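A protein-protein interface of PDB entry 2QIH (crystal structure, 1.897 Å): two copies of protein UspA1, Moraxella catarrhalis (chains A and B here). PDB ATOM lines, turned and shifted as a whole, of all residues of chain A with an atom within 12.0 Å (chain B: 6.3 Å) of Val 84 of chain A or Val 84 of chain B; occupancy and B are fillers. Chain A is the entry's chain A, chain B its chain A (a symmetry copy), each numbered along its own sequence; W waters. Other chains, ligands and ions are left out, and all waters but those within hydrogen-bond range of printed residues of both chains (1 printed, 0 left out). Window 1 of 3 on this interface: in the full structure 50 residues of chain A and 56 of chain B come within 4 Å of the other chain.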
ATOM      1  N   ARG A  75      -0.346  35.223   8.796  1.00  0.00           N
ATOM      2  CA  ARG A  75      -1.428  35.965   8.116  1.00  0.00           C
ATOM      3  C   ARG A  75      -1.851  35.291   6.824  1.00  0.00           C
ATOM      4  O   ARG A  75      -3.055  35.223   6.507  1.00  0.00           O
ATOM      5  CB  ARG A  75      -0.987  37.389   7.821  1.00  0.00           C
ATOM      6  CG  ARG A  75      -0.639  38.174   9.091  1.00  0.00           C
ATOM      7  CD  ARG A  75      -0.031  39.533   8.745  1.00  0.00           C
ATOM      8  NE  ARG A  75       0.775  40.063   9.845  1.00  0.00           N
ATOM      9  CZ  ARG A  75       1.340  41.268   9.864  1.00  0.00           C
ATOM     10  NH1 ARG A  75       1.193  42.104   8.840  1.00  0.00           N
ATOM     11  NH2 ARG A  75       2.054  41.641  10.917  1.00  0.00           N
ATOM     12  N   ALA A  76      -0.862  34.810   6.072  1.00  0.00           N
ATOM     13  CA  ALA A  76      -1.120  34.058   4.859  1.00  0.00           C
ATOM     14  C   ALA A  76      -1.848  32.756   5.182  1.00  0.00           C
ATOM     15  O   ALA A  76      -2.799  32.387   4.487  1.00  0.00           O
ATOM     16  CB  ALA A  76       0.191  33.748   4.137  1.00  0.00           C
ATOM     17  N   VAL A  77      -1.360  32.047   6.191  1.00  0.00           N
ATOM     18  CA  VAL A  77      -1.965  30.781   6.633  1.00  0.00           C
ATOM     19  C   VAL A  77      -3.431  31.008   7.051  1.00  0.00           C
ATOM     20  O   VAL A  77      -4.314  30.207   6.675  1.00  0.00           O
ATOM     21  CB  VAL A  77      -1.140  30.104   7.743  1.00  0.00           C
ATOM     22  CG1 VAL A  77      -1.822  28.821   8.279  1.00  0.00           C
ATOM     23  CG2 VAL A  77       0.239  29.742   7.204  1.00  0.00           C
ATOM     24  N   GLY A  78      -3.677  32.085   7.801  1.00  0.00           N
ATOM     25  CA  GLY A  78      -5.028  32.499   8.197  1.00  0.00           C
ATOM     26  C   GLY A  78      -5.963  32.608   7.002  1.00  0.00           C
ATOM     27  O   GLY A  78      -7.080  32.090   7.025  1.00  0.00           O
ATOM     28  N   ASN A  79      -5.471  33.231   5.939  1.00  0.00           N
ATOM     29  CA  ASN A  79      -6.270  33.450   4.745  1.00  0.00           C
ATOM     30  C   ASN A  79      -6.543  32.105   4.047  1.00  0.00           C
ATOM     31  O   ASN A  79      -7.661  31.846   3.561  1.00  0.00           O
ATOM     32  CB  ASN A  79      -5.521  34.342   3.802  1.00  0.00           C
ATOM     33  CG  ASN A  79      -5.586  35.810   4.184  1.00  0.00           C
ATOM     34  OD1 ASN A  79      -6.389  36.226   5.034  1.00  0.00           O
ATOM     35  ND2 ASN A  79      -4.726  36.618   3.534  1.00  0.00           N
ATOM     36  N   ASN A  80      -5.516  31.252   4.003  1.00  0.00           N
ATOM     37  CA  ASN A  80      -5.664  29.938   3.412  1.00  0.00           C
ATOM     38  C   ASN A  80      -6.643  29.067   4.212  1.00  0.00           C
ATOM     39  O   ASN A  80      -7.465  28.353   3.635  1.00  0.00           O
ATOM     40  CB  ASN A  80      -4.321  29.233   3.282  1.00  0.00           C
ATOM     41  CG  ASN A  80      -3.483  29.779   2.161  1.00  0.00           C
ATOM     42  OD1 ASN A  80      -3.945  30.577   1.347  1.00  0.00           O
ATOM     43  ND2 ASN A  80      -2.236  29.333   2.097  1.00  0.00           N
ATOM     44  N   THR A  81      -6.552  29.099   5.528  1.00  0.00           N
ATOM     45  CA  THR A  81      -7.477  28.285   6.327  1.00  0.00           C
ATOM     46  C   THR A  81      -8.930  28.680   6.019  1.00  0.00           C
ATOM     47  O   THR A  81      -9.798  27.810   5.818  1.00  0.00           O
ATOM     48  CB  THR A  81      -7.198  28.421   7.843  1.00  0.00           C
ATOM     49  OG1 THR A  81      -5.846  28.045   8.107  1.00  0.00           O
ATOM     50  CG2 THR A  81      -8.122  27.496   8.630  1.00  0.00           C
ATOM     51  N   GLN A  82      -9.188  29.984   5.991  1.00  0.00           N
ATOM     52  CA  GLN A  82     -10.485  30.530   5.583  1.00  0.00           C
ATOM     53  C   GLN A  82     -10.897  30.082   4.174  1.00  0.00           C
ATOM     54  O   GLN A  82     -12.076  29.786   3.937  1.00  0.00           O
ATOM     55  CB  GLN A  82     -10.436  32.050   5.582  1.00  0.00           C
ATOM     56  CG  GLN A  82     -10.326  32.670   6.969  1.00  0.00           C
ATOM     57  CD  GLN A  82     -10.193  34.189   6.944  1.00  0.00           C
ATOM     58  OE1 GLN A  82      -9.515  34.772   7.790  1.00  0.00           O
ATOM     59  NE2 GLN A  82     -10.842  34.834   5.978  1.00  0.00           N
ATOM     60  N   GLY A  83      -9.938  30.075   3.247  1.00  0.00           N
ATOM     61  CA  GLY A  83     -10.210  29.778   1.840  1.00  0.00           C
ATOM     62  C   GLY A  83     -10.554  28.309   1.678  1.00  0.00           C
ATOM     63  O   GLY A  83     -11.445  27.960   0.933  1.00  0.00           O
ATOM     64  N   VAL A  84      -9.834  27.457   2.393  1.00  0.00           N
ATOM     65  CA  VAL A  84     -10.133  26.033   2.413  1.00  0.00           C
ATOM     66  C   VAL A  84     -11.577  25.802   2.891  1.00  0.00           C
ATOM     67  O   VAL A  84     -12.329  25.107   2.218  1.00  0.00           O
ATOM     68  CB  VAL A  84      -9.109  25.219   3.219  1.00  0.00           C
ATOM     69  CG1 VAL A  84      -9.632  23.763   3.501  1.00  0.00           C
ATOM     70  CG2 VAL A  84      -7.742  25.181   2.486  1.00  0.00           C
ATOM     71  N   ALA A  85     -11.958  26.413   4.020  1.00  0.00           N
ATOM     72  CA  ALA A  85     -13.276  26.192   4.628  1.00  0.00           C
ATOM     73  C   ALA A  85     -14.383  26.689   3.702  1.00  0.00           C
ATOM     74  O   ALA A  85     -15.399  26.009   3.501  1.00  0.00           O
ATOM     75  CB  ALA A  85     -13.361  26.888   6.019  1.00  0.00           C
ATOM     76  N   THR A  86     -14.178  27.874   3.151  1.00  0.00           N
ATOM     77  CA  THR A  86     -15.089  28.444   2.173  1.00  0.00           C
ATOM     78  C   THR A  86     -15.261  27.549   0.931  1.00  0.00           C
ATOM     79  O   THR A  86     -16.387  27.255   0.506  1.00  0.00           O
ATOM     80  CB  THR A  86     -14.617  29.866   1.764  1.00  0.00           C
ATOM     81  OG1 THR A  86     -14.786  30.742   2.887  1.00  0.00           O
ATOM     82  CG2 THR A  86     -15.470  30.399   0.604  1.00  0.00           C
ATOM     83  N   ASN A  87     -14.144  27.116   0.366  1.00  0.00           N
ATOM     84  CA  ASN A  87     -14.170  26.228  -0.798  1.00  0.00           C
ATOM     85  C   ASN A  87     -14.904  24.917  -0.485  1.00  0.00           C
ATOM     86  O   ASN A  87     -15.669  24.411  -1.325  1.00  0.00           O
ATOM     87  CB  ASN A  87     -12.742  25.967  -1.321  1.00  0.00           C
ATOM     88  CG  ASN A  87     -12.192  27.147  -2.121  1.00  0.00           C
ATOM     89  OD1 ASN A  87     -12.940  28.078  -2.457  1.00  0.00           O
ATOM     90  ND2 ASN A  87     -10.875  27.116  -2.427  1.00  0.00           N
ATOM     91  N   LYS A  88     -14.667  24.402   0.725  1.00  0.00           N
ATOM     92  CA  LYS A  88     -15.279  23.141   1.187  1.00  0.00           C
ATOM     93  C   LYS A  88     -16.816  23.245   1.242  1.00  0.00           C
ATOM     94  O   LYS A  88     -17.534  22.364   0.771  1.00  0.00           O
ATOM     95  CB  LYS A  88     -14.716  22.762   2.552  1.00  0.00           C
ATOM     96  CG  LYS A  88     -15.358  21.541   3.198  1.00  0.00           C
ATOM     97  CD  LYS A  88     -14.667  21.195   4.529  1.00  0.00           C
ATOM     98  CE  LYS A  88     -15.383  20.052   5.262  1.00  0.00           C
ATOM     99  NZ  LYS A  88     -15.479  18.772   4.449  1.00  0.00           N
ATOM    100  N   ALA A  89     -17.305  24.336   1.809  1.00  0.00           N
ATOM    101  CA  ALA A  89     -18.752  24.608   1.843  1.00  0.00           C
ATOM    102  C   ALA A  89     -19.382  24.766   0.441  1.00  0.00           C
ATOM    103  O   ALA A  89     -20.448  24.217   0.180  1.00  0.00           O
ATOM    104  CB  ALA A  89     -19.017  25.824   2.676  1.00  0.00           C
ATOM    105  N   ASP A  90     -18.696  25.495  -0.441  1.00  0.00           N
ATOM    106  CA  ASP A  90     -19.138  25.733  -1.817  1.00  0.00           C
ATOM    107  C   ASP A  90     -19.186  24.442  -2.663  1.00  0.00           C
ATOM    108  O   ASP A  90     -20.128  24.240  -3.451  1.00  0.00           O
ATOM    109  CB  ASP A  90     -18.243  26.790  -2.491  1.00  0.00           C
ATOM    110  CG  ASP A  90     -18.461  28.197  -1.931  1.00  0.00           C
ATOM    111  OD1 ASP A  90     -19.358  28.361  -1.080  1.00  0.00           O
ATOM    112  OD2 ASP A  90     -17.762  29.141  -2.386  1.00  0.00           O
ATOM    113  N   ILE A  91     -18.178  23.592  -2.508  1.00  0.00           N
ATOM    114  CA  ILE A  91     -18.142  22.253  -3.113  1.00  0.00           C
ATOM    115  C   ILE A  91     -19.321  21.397  -2.642  1.00  0.00           C
ATOM    116  O   ILE A  91     -19.990  20.705  -3.442  1.00  0.00           O
ATOM    117  CB  ILE A  91     -16.803  21.534  -2.770  1.00  0.00           C
ATOM    118  CG1 ILE A  91     -15.636  22.237  -3.444  1.00  0.00           C
ATOM    119  CG2 ILE A  91     -16.853  20.045  -3.174  1.00  0.00           C
ATOM    120  CD1 ILE A  91     -14.275  21.853  -2.872  1.00  0.00           C
ATOM    121  N   ALA A  92     -19.586  21.457  -1.334  1.00  0.00           N
ATOM    122  CA  ALA A  92     -20.673  20.708  -0.751  1.00  0.00           C
ATOM    123  C   ALA A  92     -22.029  21.109  -1.339  1.00  0.00           C
ATOM    124  O   ALA A  92     -22.858  20.229  -1.608  1.00  0.00           O
ATOM    125  CB  ALA A  92     -20.683  20.853   0.732  1.00  0.00           C
ATOM    126  N   LYS A  93     -22.233  22.420  -1.525  1.00  0.00           N
ATOM    127  CA  LYS A  93     -23.422  22.979  -2.183  1.00  0.00           C
ATOM    128  C   LYS A  93     -23.529  22.491  -3.616  1.00  0.00           C
ATOM    129  O   LYS A  93     -24.606  22.088  -4.068  1.00  0.00           O
ATOM    130  CB  LYS A  93     -23.356  24.514  -2.237  1.00  0.00           C
ATOM    131  CG  LYS A  93     -23.410  25.259  -0.943  1.00  0.00           C
ATOM    132  CD  LYS A  93     -22.944  26.703  -1.191  1.00  0.00           C
ATOM    133  CE  LYS A  93     -23.318  27.619  -0.061  1.00  0.00           C
ATOM    134  NZ  LYS A  93     -23.452  29.037  -0.560  1.00  0.00           N
ATOM    135  N   ASN A  94     -22.414  22.601  -4.343  1.00  0.00           N
ATOM    136  CA  ASN A  94     -22.325  22.063  -5.688  1.00  0.00           C
ATOM    137  C   ASN A  94     -22.710  20.588  -5.770  1.00  0.00           C
ATOM    138  O   ASN A  94     -23.560  20.192  -6.590  1.00  0.00           O
ATOM    139  CB  ASN A  94     -20.935  22.320  -6.263  1.00  0.00           C
ATOM    140  CG  ASN A  94     -20.762  23.759  -6.720  1.00  0.00           C
ATOM    141  OD1 ASN A  94     -21.700  24.565  -6.631  1.00  0.00           O
ATOM    142  ND2 ASN A  94     -19.558  24.098  -7.185  1.00  0.00           N
ATOM    143  N   ASN B  79      -2.799  20.938   7.834  1.00  0.00           N
ATOM    144  CA  ASN B  79      -4.236  20.767   7.703  1.00  0.00           C
ATOM    145  C   ASN B  79      -4.720  21.412   6.391  1.00  0.00           C
ATOM    146  O   ASN B  79      -5.574  20.853   5.676  1.00  0.00           O
ATOM    147  CB  ASN B  79      -4.923  21.437   8.855  1.00  0.00           C
ATOM    148  CG  ASN B  79      -4.886  20.622  10.135  1.00  0.00           C
ATOM    149  OD1 ASN B  79      -4.547  19.427  10.135  1.00  0.00           O
ATOM    150  ND2 ASN B  79      -5.250  21.279  11.253  1.00  0.00           N
ATOM    151  N   ASN B  80      -4.166  22.587   6.080  1.00  0.00           N
ATOM    152  CA  ASN B  80      -4.509  23.268   4.849  1.00  0.00           C
ATOM    153  C   ASN B  80      -4.049  22.473   3.618  1.00  0.00           C
ATOM    154  O   ASN B  80      -4.775  22.374   2.627  1.00  0.00           O
ATOM    155  CB  ASN B  80      -3.926  24.674   4.812  1.00  0.00           C
ATOM    156  CG  ASN B  80      -4.669  25.635   5.695  1.00  0.00           C
ATOM    157  OD1 ASN B  80      -5.734  25.325   6.225  1.00  0.00           O
ATOM    158  ND2 ASN B  80      -4.116  26.831   5.846  1.00  0.00           N
ATOM    159  N   THR B  81      -2.849  21.925   3.659  1.00  0.00           N
ATOM    160  CA  THR B  81      -2.379  21.152   2.503  1.00  0.00           C
ATOM    161  C   THR B  81      -3.339  19.984   2.223  1.00  0.00           C
ATOM    162  O   THR B  81      -3.721  19.738   1.064  1.00  0.00           O
ATOM    163  CB  THR B  81      -0.941  20.618   2.716  1.00  0.00           C
ATOM    164  OG1 THR B  81      -0.067  21.719   2.970  1.00  0.00           O
ATOM    165  CG2 THR B  81      -0.460  19.895   1.462  1.00  0.00           C
ATOM    166  N   GLN B  82      -3.715  19.270   3.280  1.00  0.00           N
ATOM    167  CA  GLN B  82      -4.727  18.211   3.206  1.00  0.00           C
ATOM    168  C   GLN B  82      -6.067  18.714   2.652  1.00  0.00           C
ATOM    169  O   GLN B  82      -6.720  18.009   1.873  1.00  0.00           O
ATOM    170  CB  GLN B  82      -4.990  17.643   4.591  1.00  0.00           C
ATOM    171  CG  GLN B  82      -3.829  16.843   5.166  1.00  0.00           C
ATOM    172  CD  GLN B  82      -4.078  16.351   6.588  1.00  0.00           C
ATOM    173  OE1 GLN B  82      -3.150  16.265   7.393  1.00  0.00           O
ATOM    174  NE2 GLN B  82      -5.329  16.024   6.901  1.00  0.00           N
ATOM    175  N   GLY B  83      -6.483  19.904   3.089  1.00  0.00           N
ATOM    176  CA  GLY B  83      -7.791  20.457   2.732  1.00  0.00           C
ATOM    177  C   GLY B  83      -7.806  20.846   1.267  1.00  0.00           C
ATOM    178  O   GLY B  83      -8.779  20.623   0.576  1.00  0.00           O
ATOM    179  N   VAL B  84      -6.710  21.429   0.804  1.00  0.00           N
ATOM    180  CA  VAL B  84      -6.553  21.753  -0.605  1.00  0.00           C
ATOM    181  C   VAL B  84      -6.695  20.481  -1.460  1.00  0.00           C
ATOM    182  O   VAL B  84      -7.480  20.474  -2.402  1.00  0.00           O
ATOM    183  CB  VAL B  84      -5.253  22.518  -0.901  1.00  0.00           C
ATOM    184  CG1 VAL B  84      -4.952  22.557  -2.444  1.00  0.00           C
ATOM    185  CG2 VAL B  84      -5.320  23.953  -0.316  1.00  0.00           C
ATOM    186  N   ALA B  85      -5.967  19.415  -1.103  1.00  0.00           N
ATOM    187  CA  ALA B  85      -5.942  18.179  -1.897  1.00  0.00           C
ATOM    188  C   ALA B  85      -7.324  17.530  -1.920  1.00  0.00           C
ATOM    189  O   ALA B  85      -7.804  17.091  -2.973  1.00  0.00           O
ATOM    190  CB  ALA B  85      -4.874  17.193  -1.340  1.00  0.00           C
ATOM    191  N   THR B  86      -7.947  17.472  -0.754  1.00  0.00           N
ATOM    192  CA  THR B  86      -9.305  16.972  -0.624  1.00  0.00           C
ATOM    193  C   THR B  86     -10.313  17.767  -1.477  1.00  0.00           C
ATOM    194  O   THR B  86     -11.111  17.189  -2.228  1.00  0.00           O
ATOM    195  CB  THR B  86      -9.734  16.964   0.869  1.00  0.00           C
ATOM    196  OG1 THR B  86      -8.973  15.963   1.556  1.00  0.00           O
ATOM    197  CG2 THR B  86     -11.223  16.611   0.995  1.00  0.00           C
ATOM    198  N   ASN B  87     -10.263  19.086  -1.359  1.00  0.00           N
ATOM    199  CA  ASN B  87     -11.142  19.957  -2.143  1.00  0.00           C
ATOM    200  C   ASN B  87     -10.929  19.757  -3.650  1.00  0.00           C
ATOM    201  O   ASN B  87     -11.902  19.740  -4.423  1.00  0.00           O
ATOM    202  CB  ASN B  87     -10.954  21.433  -1.736  1.00  0.00           C
ATOM    203  CG  ASN B  87     -11.652  21.765  -0.417  1.00  0.00           C
ATOM    204  OD1 ASN B  87     -12.439  20.954   0.095  1.00  0.00           O
ATOM    205  ND2 ASN B  87     -11.362  22.961   0.143  1.00  0.00           N
ATOM    206  N   LYS B  88      -9.659  19.592  -4.033  1.00  0.00           N
ATOM    207  CA  LYS B  88      -9.272  19.400  -5.444  1.00  0.00           C
ATOM    208  C   LYS B  88      -9.891  18.117  -6.031  1.00  0.00           C
ATOM    209  O   LYS B  88     -10.448  18.117  -7.127  1.00  0.00           O
ATOM    210  CB  LYS B  88      -7.753  19.369  -5.565  1.00  0.00           C
ATOM    211  CG  LYS B  88      -7.223  19.052  -6.958  1.00  0.00           C
ATOM    212  CD  LYS B  88      -5.686  19.124  -6.991  1.00  0.00           C
ATOM    213  CE  LYS B  88      -5.125  18.677  -8.349  1.00  0.00           C
ATOM    214  NZ  LYS B  88      -5.648  19.489  -9.522  1.00  0.00           N
ATOM    215  N   ALA B  89      -9.798  17.030  -5.279  1.00  0.00           N
ATOM    216  CA  ALA B  89     -10.428  15.760  -5.675  1.00  0.00           C
ATOM    217  C   ALA B  89     -11.968  15.843  -5.781  1.00  0.00           C
ATOM    218  O   ALA B  89     -12.547  15.340  -6.739  1.00  0.00           O
ATOM    219  CB  ALA B  89     -10.028  14.679  -4.718  1.00  0.00           C
HETATM  220  O   HOH W   1      -5.233  25.326   9.090  1.00  0.00           O
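The side-chain amide nitrogen (ND2) of Asn 80 of chain B lies within hydrogen-bond range of the backbone carbonyl oxygen (O) of Val 77 of chain A. The side-chain amide nitrogen (ND2) of Asn 80 of chain B is in hydrogen-bond range of the side-chain hydroxyl (OG1) of Thr 81 of chain A (3.1 Å). ND2 of Asn 87 of chain B lies within hydrogen-bond range of O of Val 84 of chain A (3.1 Å).
The backbone carbonyl oxygen (O) of Val 77 of chain A lies within hydrogen-bond range of the side-chain hydroxyl (OG1) of Thr 81 of chain A.
Among the printed residues, merely in contact across the chains: Asn 80 of chain A with Asn 80 of chain B, Val 84 of chain A with Gly 83 of chain B, Val 84 of chain A with Val 84 of chain B, Asn 87 of chain A with Asn 87 of chain B, Lys 88 of chain A with Asn 87 of chain B and Ile 91 of chain A with Asn 87 of chain B.
Printed residues of chain B within 4 Å of Val 84 of chain A: Gly 83, Val 84 and Asn 87. Val 84 of chain B touches just one residue of chain A: Val 84. Of chain A, only Val 77 (3.5 Å), Asn 80 (3.5 Å) and Thr 81 (3.1 Å) come within 4 Å of Asn 80 of chain B. No residue of chain A comes within 4 Å of Thr 81 of chain B. Gly 83 of chain B touches just one residue of chain A: Val 84 (3.9 Å). No residue of chain A comes within 4 Å of Ala 85 of chain B. Asn 87 of chain B touches four residues of chain A. No residue of chain A comes within 4 Å of Lys 88 of chain B. Of the printed residues of chain B, Val 77 of chain A touches Asn 80. Of the printed residues of chain B, Thr 81 of chain A touches Asn 80. Asp 90 of chain A touches none of the printed residues of chain B. Lys 93 of chain A touches none of the printed residues of chain B. The nearest residue of chain B that does not touch Val 84 of chain A is Asn 80 of chain B (4.1 Å). The nearest residue of chain A that does not touch Val 84 of chain B is Asn 80 of chain A (6.3 Å). The nearest printed residue of chain B that does not touch Asn 87 of chain A is Val 84 of chain B (6.7 Å).
Of the 20 printed residues of chain A, 7 touch a printed residue of chain B. Printed residues of chain A that touch a printed residue of chain B: Val 77, Asn 80, Thr 81, Val 84, Asn 87, Lys 88 and Ile 91. Of the 11 printed residues of chain B, 4 touch a printed residue of chain A. Hydrophobic or aromatic side chains of chain B within 4 Å of the printed part of chain A: Val 84. Among the printed residues, 9 pairs touch across the chains. Among the printed residues, no Asp or Glu carboxylate lies within 4 Å of a Lys or Arg side-chain nitrogen of the other chain.
Asn 80 of chain B touches its own counterpart, Asn 80 of chain A. Thr 81 of chain A touches Asn 80 of chain B, but with the chains exchanged Asn 80 of chain A does not touch Thr 81 of chain B (7.5 Å). Val 84 of chain A touches Gly 83 of chain B, but with the chains exchanged Gly 83 of chain A does not touch Val 84 of chain B (7.1 Å). Val 84 of chain A touches Asn 87 of chain B, but with the chains exchanged Asn 87 of chain A does not touch Val 84 of chain B (6.7 Å). Positions printed for both chains: 79, 80, 81, 82, 83, 84, 85, 86, 87, 88 and 89. Of the 9 pairs that touch across the chains among the printed residues, 3 have their exchanged pair printed and touching as well.
Water W1 bridges the side-chain amide oxygen (OD1) of Asn 80 of chain B (2.9 Å) and the side-chain hydroxyl (OG1) of Thr 81 of chain A (3.0 Å).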
